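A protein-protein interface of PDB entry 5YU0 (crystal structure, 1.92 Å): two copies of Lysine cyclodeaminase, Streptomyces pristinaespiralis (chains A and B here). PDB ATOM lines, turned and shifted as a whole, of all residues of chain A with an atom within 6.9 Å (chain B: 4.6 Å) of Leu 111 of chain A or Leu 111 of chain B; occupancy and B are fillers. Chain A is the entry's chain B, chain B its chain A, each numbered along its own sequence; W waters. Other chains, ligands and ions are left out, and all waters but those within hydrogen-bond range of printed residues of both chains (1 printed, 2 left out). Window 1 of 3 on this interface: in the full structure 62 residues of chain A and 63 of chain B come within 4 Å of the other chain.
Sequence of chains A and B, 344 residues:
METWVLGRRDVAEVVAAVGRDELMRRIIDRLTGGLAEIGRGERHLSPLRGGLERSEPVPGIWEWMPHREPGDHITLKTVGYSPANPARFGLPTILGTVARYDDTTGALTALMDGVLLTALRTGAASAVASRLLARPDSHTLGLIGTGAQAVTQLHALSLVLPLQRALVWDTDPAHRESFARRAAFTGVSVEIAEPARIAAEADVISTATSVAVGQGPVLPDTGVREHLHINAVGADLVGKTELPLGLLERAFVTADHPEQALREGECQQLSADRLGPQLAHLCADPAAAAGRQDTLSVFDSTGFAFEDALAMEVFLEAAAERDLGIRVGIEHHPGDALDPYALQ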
ATOM      1  N   THR A   3      16.394  15.470  -8.916  1.00  0.00           N
ATOM      2  CA  THR A   3      15.065  15.792  -8.416  1.00  0.00           C
ATOM      3  C   THR A   3      15.176  16.515  -7.078  1.00  0.00           C
ATOM      4  O   THR A   3      15.914  16.082  -6.186  1.00  0.00           O
ATOM      5  CB  THR A   3      14.234  14.524  -8.258  1.00  0.00           C
ATOM      6  OG1 THR A   3      14.083  13.891  -9.536  1.00  0.00           O
ATOM      7  CG2 THR A   3      12.846  14.869  -7.683  1.00  0.00           C
ATOM      8  N   TRP A   4      14.460  17.628  -6.957  1.00  0.00           N
ATOM      9  CA  TRP A   4      14.369  18.365  -5.704  1.00  0.00           C
ATOM     10  C   TRP A   4      13.294  17.718  -4.833  1.00  0.00           C
ATOM     11  O   TRP A   4      12.128  17.636  -5.232  1.00  0.00           O
ATOM     12  CB  TRP A   4      14.060  19.830  -6.009  1.00  0.00           C
ATOM     13  CG  TRP A   4      14.032  20.754  -4.828  1.00  0.00           C
ATOM     14  CD1 TRP A   4      14.591  20.556  -3.590  1.00  0.00           C
ATOM     15  CD2 TRP A   4      13.400  22.033  -4.785  1.00  0.00           C
ATOM     16  NE1 TRP A   4      14.340  21.644  -2.782  1.00  0.00           N
ATOM     17  CE2 TRP A   4      13.611  22.564  -3.492  1.00  0.00           C
ATOM     18  CE3 TRP A   4      12.674  22.785  -5.719  1.00  0.00           C
ATOM     19  CZ2 TRP A   4      13.119  23.814  -3.108  1.00  0.00           C
ATOM     20  CZ3 TRP A   4      12.184  24.029  -5.335  1.00  0.00           C
ATOM     21  CH2 TRP A   4      12.415  24.530  -4.040  1.00  0.00           C
ATOM     22  N   VAL A   5      13.688  17.201  -3.672  1.00  0.00           N
ATOM     23  CA  VAL A   5      12.774  16.497  -2.778  1.00  0.00           C
ATOM     24  C   VAL A   5      12.596  17.330  -1.521  1.00  0.00           C
ATOM     25  O   VAL A   5      13.577  17.642  -0.833  1.00  0.00           O
ATOM     26  CB  VAL A   5      13.278  15.088  -2.428  1.00  0.00           C
ATOM     27  CG1 VAL A   5      12.279  14.386  -1.511  1.00  0.00           C
ATOM     28  CG2 VAL A   5      13.495  14.274  -3.698  1.00  0.00           C
ATOM     29  N   LEU A   6      11.347  17.694  -1.227  1.00  0.00           N
ATOM     30  CA  LEU A   6      10.984  18.324   0.040  1.00  0.00           C
ATOM     31  C   LEU A   6      10.416  17.245   0.949  1.00  0.00           C
ATOM     32  O   LEU A   6       9.310  16.744   0.712  1.00  0.00           O
ATOM     33  CB  LEU A   6       9.973  19.449  -0.164  1.00  0.00           C
ATOM     34  CG  LEU A   6      10.420  20.615  -1.037  1.00  0.00           C
ATOM     35  CD1 LEU A   6       9.302  21.656  -1.151  1.00  0.00           C
ATOM     36  CD2 LEU A   6      11.685  21.236  -0.463  1.00  0.00           C
ATOM     37  N   GLY A   7      11.166  16.884   1.982  1.00  0.00           N
ATOM     38  CA  GLY A   7      10.709  15.899   2.936  1.00  0.00           C
ATOM     39  C   GLY A   7       9.786  16.488   3.990  1.00  0.00           C
ATOM     40  O   GLY A   7       9.480  17.684   4.008  1.00  0.00           O
ATOM     41  N   LEU A  76       1.474  15.695 -10.714  1.00  0.00           N
ATOM     42  CA  LEU A  76       0.707  14.490 -10.430  1.00  0.00           C
ATOM     43  C   LEU A  76       0.644  14.289  -8.925  1.00  0.00           C
ATOM     44  O   LEU A  76       1.685  14.176  -8.265  1.00  0.00           O
ATOM     45  CB  LEU A  76       1.321  13.261 -11.100  1.00  0.00           C
ATOM     46  CG  LEU A  76       0.565  11.990 -10.709  1.00  0.00           C
ATOM     47  CD1 LEU A  76      -0.632  11.835 -11.606  1.00  0.00           C
ATOM     48  CD2 LEU A  76       1.482  10.783 -10.794  1.00  0.00           C
ATOM     49  N   THR A  78      -0.588  11.623  -6.069  1.00  0.00           N
ATOM     50  CA  THR A  78      -1.032  10.272  -5.760  1.00  0.00           C
ATOM     51  C   THR A  78      -1.487  10.290  -4.314  1.00  0.00           C
ATOM     52  O   THR A  78      -0.740  10.748  -3.448  1.00  0.00           O
ATOM     53  CB  THR A  78       0.098   9.253  -5.939  1.00  0.00           C
ATOM     54  OG1 THR A  78       1.298   9.771  -5.344  1.00  0.00           O
ATOM     55  CG2 THR A  78       0.355   8.997  -7.426  1.00  0.00           C
ATOM     56  N   THR A  97       1.387  12.201  -1.981  1.00  0.00           N
ATOM     57  CA  THR A  97       2.608  12.858  -2.422  1.00  0.00           C
ATOM     58  C   THR A  97       2.316  13.579  -3.733  1.00  0.00           C
ATOM     59  O   THR A  97       1.423  13.191  -4.491  1.00  0.00           O
ATOM     60  CB  THR A  97       3.772  11.852  -2.602  1.00  0.00           C
ATOM     61  OG1 THR A  97       3.278  10.647  -3.190  1.00  0.00           O
ATOM     62  CG2 THR A  97       4.397  11.490  -1.246  1.00  0.00           C
ATOM     63  N   VAL A  98       3.073  14.638  -3.997  1.00  0.00           N
ATOM     64  CA  VAL A  98       2.891  15.450  -5.190  1.00  0.00           C
ATOM     65  C   VAL A  98       4.212  15.507  -5.941  1.00  0.00           C
ATOM     66  O   VAL A  98       5.246  15.867  -5.364  1.00  0.00           O
ATOM     67  CB  VAL A  98       2.404  16.867  -4.842  1.00  0.00           C
ATOM     68  CG1 VAL A  98       1.874  17.545  -6.093  1.00  0.00           C
ATOM     69  CG2 VAL A  98       1.334  16.806  -3.744  1.00  0.00           C
ATOM     70  N   ALA A  99       4.178  15.154  -7.221  1.00  0.00           N
ATOM     71  CA  ALA A  99       5.368  15.164  -8.062  1.00  0.00           C
ATOM     72  C   ALA A  99       5.205  16.200  -9.162  1.00  0.00           C
ATOM     73  O   ALA A  99       4.090  16.457  -9.629  1.00  0.00           O
ATOM     74  CB  ALA A  99       5.629  13.772  -8.678  1.00  0.00           C
ATOM     75  N   ARG A 100       6.329  16.797  -9.579  1.00  0.00           N
ATOM     76  CA  ARG A 100       6.339  17.766 -10.666  1.00  0.00           C
ATOM     77  C   ARG A 100       7.298  17.297 -11.753  1.00  0.00           C
ATOM     78  O   ARG A 100       8.442  16.930 -11.463  1.00  0.00           O
ATOM     79  CB  ARG A 100       6.742  19.168 -10.182  1.00  0.00           C
ATOM     80  CG  ARG A 100       7.055  20.127 -11.332  1.00  0.00           C
ATOM     81  CD  ARG A 100       7.239  21.567 -10.849  1.00  0.00           C
ATOM     82  NE  ARG A 100       6.023  22.062 -10.214  1.00  0.00           N
ATOM     83  CZ  ARG A 100       5.795  23.337  -9.924  1.00  0.00           C
ATOM     84  NH1 ARG A 100       6.709  24.253 -10.210  1.00  0.00           N
ATOM     85  NH2 ARG A 100       4.655  23.691  -9.338  1.00  0.00           N
ATOM     86  N   TYR A 101       6.830  17.321 -13.000  1.00  0.00           N
ATOM     87  CA  TYR A 101       7.616  16.895 -14.148  1.00  0.00           C
ATOM     88  C   TYR A 101       7.767  18.061 -15.108  1.00  0.00           C
ATOM     89  O   TYR A 101       6.815  18.813 -15.334  1.00  0.00           O
ATOM     90  CB  TYR A 101       6.964  15.704 -14.877  1.00  0.00           C
ATOM     91  CG  TYR A 101       6.647  14.551 -13.958  1.00  0.00           C
ATOM     92  CD1 TYR A 101       5.527  14.586 -13.147  1.00  0.00           C
ATOM     93  CD2 TYR A 101       7.475  13.430 -13.895  1.00  0.00           C
ATOM     94  CE1 TYR A 101       5.231  13.551 -12.292  1.00  0.00           C
ATOM     95  CE2 TYR A 101       7.189  12.380 -13.031  1.00  0.00           C
ATOM     96  CZ  TYR A 101       6.054  12.449 -12.243  1.00  0.00           C
ATOM     97  OH  TYR A 101       5.730  11.431 -11.379  1.00  0.00           O
ATOM     98  N   LEU A 108      11.441  14.292 -14.035  1.00  0.00           N
ATOM     99  CA  LEU A 108      10.947  14.516 -12.680  1.00  0.00           C
ATOM    100  C   LEU A 108      11.814  15.576 -12.004  1.00  0.00           C
ATOM    101  O   LEU A 108      12.989  15.330 -11.711  1.00  0.00           O
ATOM    102  CB  LEU A 108      10.974  13.210 -11.890  1.00  0.00           C
ATOM    103  CG  LEU A 108      10.644  13.298 -10.393  1.00  0.00           C
ATOM    104  CD1 LEU A 108       9.179  13.700 -10.211  1.00  0.00           C
ATOM    105  CD2 LEU A 108      10.941  11.982  -9.642  1.00  0.00           C
ATOM    106  N   THR A 109      11.245  16.754 -11.742  1.00  0.00           N
ATOM    107  CA  THR A 109      12.023  17.862 -11.196  1.00  0.00           C
ATOM    108  C   THR A 109      11.801  18.097  -9.708  1.00  0.00           C
ATOM    109  O   THR A 109      12.682  18.664  -9.053  1.00  0.00           O
ATOM    110  CB  THR A 109      11.711  19.164 -11.948  1.00  0.00           C
ATOM    111  OG1 THR A 109      10.320  19.473 -11.813  1.00  0.00           O
ATOM    112  CG2 THR A 109      12.063  19.033 -13.431  1.00  0.00           C
ATOM    113  N   ALA A 110      10.663  17.689  -9.156  1.00  0.00           N
ATOM    114  CA  ALA A 110      10.393  17.963  -7.754  1.00  0.00           C
ATOM    115  C   ALA A 110       9.415  16.933  -7.213  1.00  0.00           C
ATOM    116  O   ALA A 110       8.576  16.406  -7.950  1.00  0.00           O
ATOM    117  CB  ALA A 110       9.841  19.382  -7.563  1.00  0.00           C
ATOM    118  N   LEU A 111       9.529  16.667  -5.912  1.00  0.00           N
ATOM    119  CA  LEU A 111       8.668  15.719  -5.219  1.00  0.00           C
ATOM    120  C   LEU A 111       8.511  16.165  -3.771  1.00  0.00           C
ATOM    121  O   LEU A 111       9.500  16.521  -3.124  1.00  0.00           O
ATOM    122  CB  LEU A 111       9.257  14.307  -5.290  1.00  0.00           C
ATOM    123  CG  LEU A 111       8.529  13.209  -4.525  1.00  0.00           C
ATOM    124  CD1 LEU A 111       7.174  12.896  -5.197  1.00  0.00           C
ATOM    125  CD2 LEU A 111       9.408  11.961  -4.424  1.00  0.00           C
ATOM    126  N   MET A 112       7.282  16.139  -3.256  1.00  0.00           N
ATOM    127  CA  MET A 112       7.057  16.608  -1.892  1.00  0.00           C
ATOM    128  C   MET A 112       5.895  15.861  -1.258  1.00  0.00           C
ATOM    129  O   MET A 112       5.105  15.202  -1.937  1.00  0.00           O
ATOM    130  CB  MET A 112       6.785  18.119  -1.855  1.00  0.00           C
ATOM    131  CG  MET A 112       5.467  18.522  -2.528  1.00  0.00           C
ATOM    132  SD  MET A 112       5.124  20.297  -2.421  1.00  0.00           S
ATOM    133  CE  MET A 112       5.006  20.452  -0.649  1.00  0.00           C
ATOM    134  N   ASP A 113       5.806  15.985   0.066  1.00  0.00           N
ATOM    135  CA  ASP A 113       4.644  15.516   0.805  1.00  0.00           C
ATOM    136  C   ASP A 113       3.367  16.112   0.226  1.00  0.00           C
ATOM    137  O   ASP A 113       3.332  17.280  -0.174  1.00  0.00           O
ATOM    138  CB  ASP A 113       4.775  15.912   2.280  1.00  0.00           C
ATOM    139  CG  ASP A 113       3.488  15.773   3.039  1.00  0.00           C
ATOM    140  OD1 ASP A 113       2.996  14.635   3.149  1.00  0.00           O
ATOM    141  OD2 ASP A 113       2.966  16.803   3.528  1.00  0.00           O
ATOM    142  N   MET A 312       1.492  23.460  -4.537  1.00  0.00           N
ATOM    143  CA  MET A 312       2.889  23.036  -4.601  1.00  0.00           C
ATOM    144  C   MET A 312       3.800  24.205  -4.972  1.00  0.00           C
ATOM    145  O   MET A 312       4.892  24.352  -4.410  1.00  0.00           O
ATOM    146  CB  MET A 312       3.040  21.886  -5.599  1.00  0.00           C
ATOM    147  CG  MET A 312       4.489  21.432  -5.799  1.00  0.00           C
ATOM    148  SD  MET A 312       4.568  19.698  -6.311  1.00  0.00           S
ATOM    149  CE  MET A 312       6.357  19.403  -6.297  1.00  0.00           C
ATOM    150  N   LEU A 316       7.119  25.460  -3.065  1.00  0.00           N
ATOM    151  CA  LEU A 316       8.431  25.493  -3.716  1.00  0.00           C
ATOM    152  C   LEU A 316       9.040  26.889  -3.660  1.00  0.00           C
ATOM    153  O   LEU A 316      10.255  27.036  -3.461  1.00  0.00           O
ATOM    154  CB  LEU A 316       8.330  25.011  -5.168  1.00  0.00           C
ATOM    155  CG  LEU A 316       7.899  23.547  -5.371  1.00  0.00           C
ATOM    156  CD1 LEU A 316       7.841  23.194  -6.856  1.00  0.00           C
ATOM    157  CD2 LEU A 316       8.828  22.598  -4.621  1.00  0.00           C
ATOM    158  N   ILE A 330      17.284  10.552  -9.187  1.00  0.00           N
ATOM    159  CA  ILE A 330      16.398   9.391  -9.254  1.00  0.00           C
ATOM    160  C   ILE A 330      16.359   8.810 -10.659  1.00  0.00           C
ATOM    161  O   ILE A 330      16.595   7.617 -10.851  1.00  0.00           O
ATOM    162  CB  ILE A 330      14.982   9.765  -8.761  1.00  0.00           C
ATOM    163  CG1 ILE A 330      15.045  10.312  -7.331  1.00  0.00           C
ATOM    164  CG2 ILE A 330      14.023   8.554  -8.854  1.00  0.00           C
ATOM    165  CD1 ILE A 330      13.722  10.867  -6.850  1.00  0.00           C
ATOM    166  N   THR B   3      10.134   6.451   2.860  1.00  0.00           N
ATOM    167  CA  THR B   3      10.133   5.922   1.505  1.00  0.00           C
ATOM    168  C   THR B   3      11.519   5.392   1.155  1.00  0.00           C
ATOM    169  O   THR B   3      12.526   6.072   1.367  1.00  0.00           O
ATOM    170  CB  THR B   3       9.728   7.009   0.504  1.00  0.00           C
ATOM    171  OG1 THR B   3       8.415   7.483   0.810  1.00  0.00           O
ATOM    172  CG2 THR B   3       9.750   6.464  -0.920  1.00  0.00           C
ATOM    173  N   TRP B   4      11.565   4.187   0.598  1.00  0.00           N
ATOM    174  CA  TRP B   4      12.817   3.607   0.118  1.00  0.00           C
ATOM    175  C   TRP B   4      13.076   4.128  -1.291  1.00  0.00           C
ATOM    176  O   TRP B   4      12.344   3.800  -2.227  1.00  0.00           O
ATOM    177  CB  TRP B   4      12.710   2.087   0.154  1.00  0.00           C
ATOM    178  CG  TRP B   4      13.921   1.320  -0.275  1.00  0.00           C
ATOM    179  CD1 TRP B   4      15.220   1.754  -0.324  1.00  0.00           C
ATOM    180  CD2 TRP B   4      13.931  -0.042  -0.702  1.00  0.00           C
ATOM    181  NE1 TRP B   4      16.040   0.733  -0.775  1.00  0.00           N
ATOM    182  CE2 TRP B   4      15.270  -0.378  -1.011  1.00  0.00           C
ATOM    183  CE3 TRP B   4      12.931  -1.011  -0.873  1.00  0.00           C
ATOM    184  CZ2 TRP B   4      15.631  -1.643  -1.467  1.00  0.00           C
ATOM    185  CZ3 TRP B   4      13.292  -2.269  -1.335  1.00  0.00           C
ATOM    186  CH2 TRP B   4      14.633  -2.573  -1.628  1.00  0.00           C
ATOM    187  N   VAL B   5      14.085   4.971  -1.445  1.00  0.00           N
ATOM    188  CA  VAL B   5      14.416   5.558  -2.739  1.00  0.00           C
ATOM    189  C   VAL B   5      15.633   4.839  -3.303  1.00  0.00           C
ATOM    190  O   VAL B   5      16.677   4.766  -2.648  1.00  0.00           O
ATOM    191  CB  VAL B   5      14.681   7.067  -2.615  1.00  0.00           C
ATOM    192  CG1 VAL B   5      15.002   7.662  -3.984  1.00  0.00           C
ATOM    193  CG2 VAL B   5      13.468   7.762  -1.993  1.00  0.00           C
ATOM    194  N   LEU B   6      15.494   4.300  -4.511  1.00  0.00           N
ATOM    195  CA  LEU B   6      16.623   3.769  -5.274  1.00  0.00           C
ATOM    196  C   LEU B   6      17.062   4.840  -6.267  1.00  0.00           C
ATOM    197  O   LEU B   6      16.418   5.038  -7.298  1.00  0.00           O
ATOM    198  CB  LEU B   6      16.233   2.489  -6.004  1.00  0.00           C
ATOM    199  CG  LEU B   6      15.946   1.227  -5.200  1.00  0.00           C
ATOM    200  CD1 LEU B   6      15.829   0.045  -6.164  1.00  0.00           C
ATOM    201  CD2 LEU B   6      17.052   0.992  -4.185  1.00  0.00           C
ATOM    202  N   THR B  97       9.750   7.155 -14.067  1.00  0.00           N
ATOM    203  CA  THR B  97      10.008   6.709 -12.710  1.00  0.00           C
ATOM    204  C   THR B  97       8.895   5.748 -12.317  1.00  0.00           C
ATOM    205  O   THR B  97       7.796   5.776 -12.885  1.00  0.00           O
ATOM    206  CB  THR B  97      10.079   7.901 -11.735  1.00  0.00           C
ATOM    207  OG1 THR B  97       9.087   8.861 -12.101  1.00  0.00           O
ATOM    208  CG2 THR B  97      11.447   8.591 -11.816  1.00  0.00           C
ATOM    209  N   VAL B  98       9.193   4.872 -11.358  1.00  0.00           N
ATOM    210  CA  VAL B  98       8.264   3.838 -10.919  1.00  0.00           C
ATOM    211  C   VAL B  98       8.143   3.917  -9.403  1.00  0.00           C
ATOM    212  O   VAL B  98       9.156   3.906  -8.695  1.00  0.00           O
ATOM    213  CB  VAL B  98       8.712   2.428 -11.337  1.00  0.00           C
ATOM    214  CG1 VAL B  98       7.525   1.462 -11.287  1.00  0.00           C
ATOM    215  CG2 VAL B  98       9.340   2.449 -12.738  1.00  0.00           C
ATOM    216  N   ALA B  99       6.912   3.965  -8.911  1.00  0.00           N
ATOM    217  CA  ALA B  99       6.644   4.107  -7.487  1.00  0.00           C
ATOM    218  C   ALA B  99       5.819   2.927  -6.997  1.00  0.00           C
ATOM    219  O   ALA B  99       5.063   2.314  -7.762  1.00  0.00           O
ATOM    220  CB  ALA B  99       5.907   5.431  -7.188  1.00  0.00           C
ATOM    221  N   ALA B 110       8.244   2.865  -1.951  1.00  0.00           N
ATOM    222  CA  ALA B 110       9.451   2.746  -2.761  1.00  0.00           C
ATOM    223  C   ALA B 110       9.310   3.571  -4.031  1.00  0.00           C
ATOM    224  O   ALA B 110       8.213   3.709  -4.585  1.00  0.00           O
ATOM    225  CB  ALA B 110       9.741   1.284  -3.114  1.00  0.00           C
ATOM    226  N   LEU B 111      10.444   4.107  -4.485  1.00  0.00           N
ATOM    227  CA  LEU B 111      10.529   4.947  -5.671  1.00  0.00           C
ATOM    228  C   LEU B 111      11.859   4.675  -6.370  1.00  0.00           C
ATOM    229  O   LEU B 111      12.906   4.665  -5.716  1.00  0.00           O
ATOM    230  CB  LEU B 111      10.415   6.428  -5.281  1.00  0.00           C
ATOM    231  CG  LEU B 111      10.567   7.454  -6.392  1.00  0.00           C
ATOM    232  CD1 LEU B 111       9.455   7.280  -7.418  1.00  0.00           C
ATOM    233  CD2 LEU B 111      10.543   8.860  -5.807  1.00  0.00           C
ATOM    234  N   MET B 112      11.827   4.466  -7.693  1.00  0.00           N
ATOM    235  CA  MET B 112      13.058   4.179  -8.429  1.00  0.00           C
ATOM    236  C   MET B 112      12.982   4.717  -9.852  1.00  0.00           C
ATOM    237  O   MET B 112      11.900   5.017 -10.375  1.00  0.00           O
ATOM    238  CB  MET B 112      13.349   2.675  -8.468  1.00  0.00           C
ATOM    239  CG  MET B 112      12.271   1.851  -9.207  1.00  0.00           C
ATOM    240  SD  MET B 112      12.747   0.114  -9.443  1.00  0.00           S
ATOM    241  CE  MET B 112      14.125   0.337 -10.562  1.00  0.00           C
ATOM    242  N   MET B 312      10.100  -4.090 -11.375  1.00  0.00           N
ATOM    243  CA  MET B 312      10.447  -3.402 -10.134  1.00  0.00           C
ATOM    244  C   MET B 312      10.727  -4.402  -9.016  1.00  0.00           C
ATOM    245  O   MET B 312      11.672  -4.224  -8.238  1.00  0.00           O
ATOM    246  CB  MET B 312       9.338  -2.427  -9.727  1.00  0.00           C
ATOM    247  CG  MET B 312       9.637  -1.702  -8.388  1.00  0.00           C
ATOM    248  SD  MET B 312       8.769  -0.119  -8.319  1.00  0.00           S
ATOM    249  CE  MET B 312       9.352   0.564  -6.746  1.00  0.00           C
ATOM    250  N   ILE B 330       9.266  11.392   3.187  1.00  0.00           N
ATOM    251  CA  ILE B 330       8.696  12.335   2.233  1.00  0.00           C
ATOM    252  C   ILE B 330       7.304  12.712   2.713  1.00  0.00           C
ATOM    253  O   ILE B 330       6.995  13.893   2.909  1.00  0.00           O
ATOM    254  CB  ILE B 330       8.654  11.751   0.806  1.00  0.00           C
ATOM    255  CG1 ILE B 330      10.062  11.331   0.358  1.00  0.00           C
ATOM    256  CG2 ILE B 330       8.031  12.768  -0.172  1.00  0.00           C
ATOM    257  CD1 ILE B 330      10.119  10.851  -1.078  1.00  0.00           C
HETATM  258  O   HOH W   1       7.334   9.853  -9.736  1.00  0.00           O
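Of the printed residues of chain B, Gly 7 of chain A touches Ile 330 (3.96 Å).
Of the printed residues of chain B, Met 112 of chain A touches Ile 330.
Of the printed residues of chain B, Ile 330 of chain A touches Thr 97 and Leu 111.
Printed residues of chain A within 4 Å of Thr 97 of chain B: Ile 330 (3.9 Å).
Leu 111 of chain B touches just these residues of chain A: Leu 111 (3.6 Å) and Ile 330 (3.9 Å).
Printed residues of chain A within 4 Å of Ile 330 of chain B: Gly 7 (3.96 Å), Thr 97 (3.999 Å), Leu 111 (3.6 Å), Met 112 (3.9 Å) and Asp 113 (3.1 Å).
The nearest residue of chain A that does not touch Leu 111 of chain B is Leu 108 of chain A (5.0 Å).
Thr 97 of chain A touches Ile 330 of chain B, and with the chains exchanged Ile 330 of chain A touches Thr 97 of chain B.
Leu 111 of chain B touches its own counterpart, Leu 111 of chain A.
Leu 111 of chain A touches Ile 330 of chain B, and with the chains exchanged Ile 330 of chain A touches Leu 111 of chain B.
Met 112 of chain A touches Ile 330 of chain B, but with the chains exchanged Ile 330 of chain A does not touch Met 112 of chain B (4.1 Å).
Water W1 lies within hydrogen-bond range of the side-chain hydroxyl (OH) of Tyr 101 of chain A and the side-chain hydroxyl (OG1) of Thr 97 of chain B.
The backbone NH (N) of Leu 6 of chain A is in hydrogen-bond range of the backbone carbonyl oxygen (O) of Leu 111 of chain A.
The backbone carbonyl oxygen (O) of Val 98 of chain A is in hydrogen-bond range of the backbone NH (N) of Met 112 of chain A.
The backbone carbonyl oxygen (O) of Leu 111 of chain B lies within hydrogen-bond range of the backbone NH (N) of Leu 6 of chain B, 2.9 Å away.
O of Trp 4 of chain A is in hydrogen-bond range of N of Leu 111 of chain A (2.9 Å).
The backbone carbonyl oxygen (O) of Trp 4 of chain B is in hydrogen-bond range of the backbone NH (N) of Leu 111 of chain B.
The backbone carbonyl oxygen of Thr 78 of chain A sits at hydrogen-bond distance from the backbone NH of Thr 97 of chain A, at 3.0 Å.
Of the 21 printed residues of chain A, 6 touch a printed residue of chain B.
Among the printed residues, no Asp or Glu carboxylate lies within 4 Å of a Lys or Arg side-chain nitrogen of the other chain.
Among the printed residues, merely in contact across the chains: Asp 113 of chain A with Ile 330 of chain B, Leu 111 of chain A with Leu 111 of chain B, Leu 111 of chain A with Ile 330 of chain B, Ile 330 of chain A with Leu 111 of chain B, Met 112 of chain A with Ile 330 of chain B, Ile 330 of chain A with Thr 97 of chain B, Gly 7 of chain A with Ile 330 of chain B and Thr 97 of chain A with Ile 330 of chain B.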
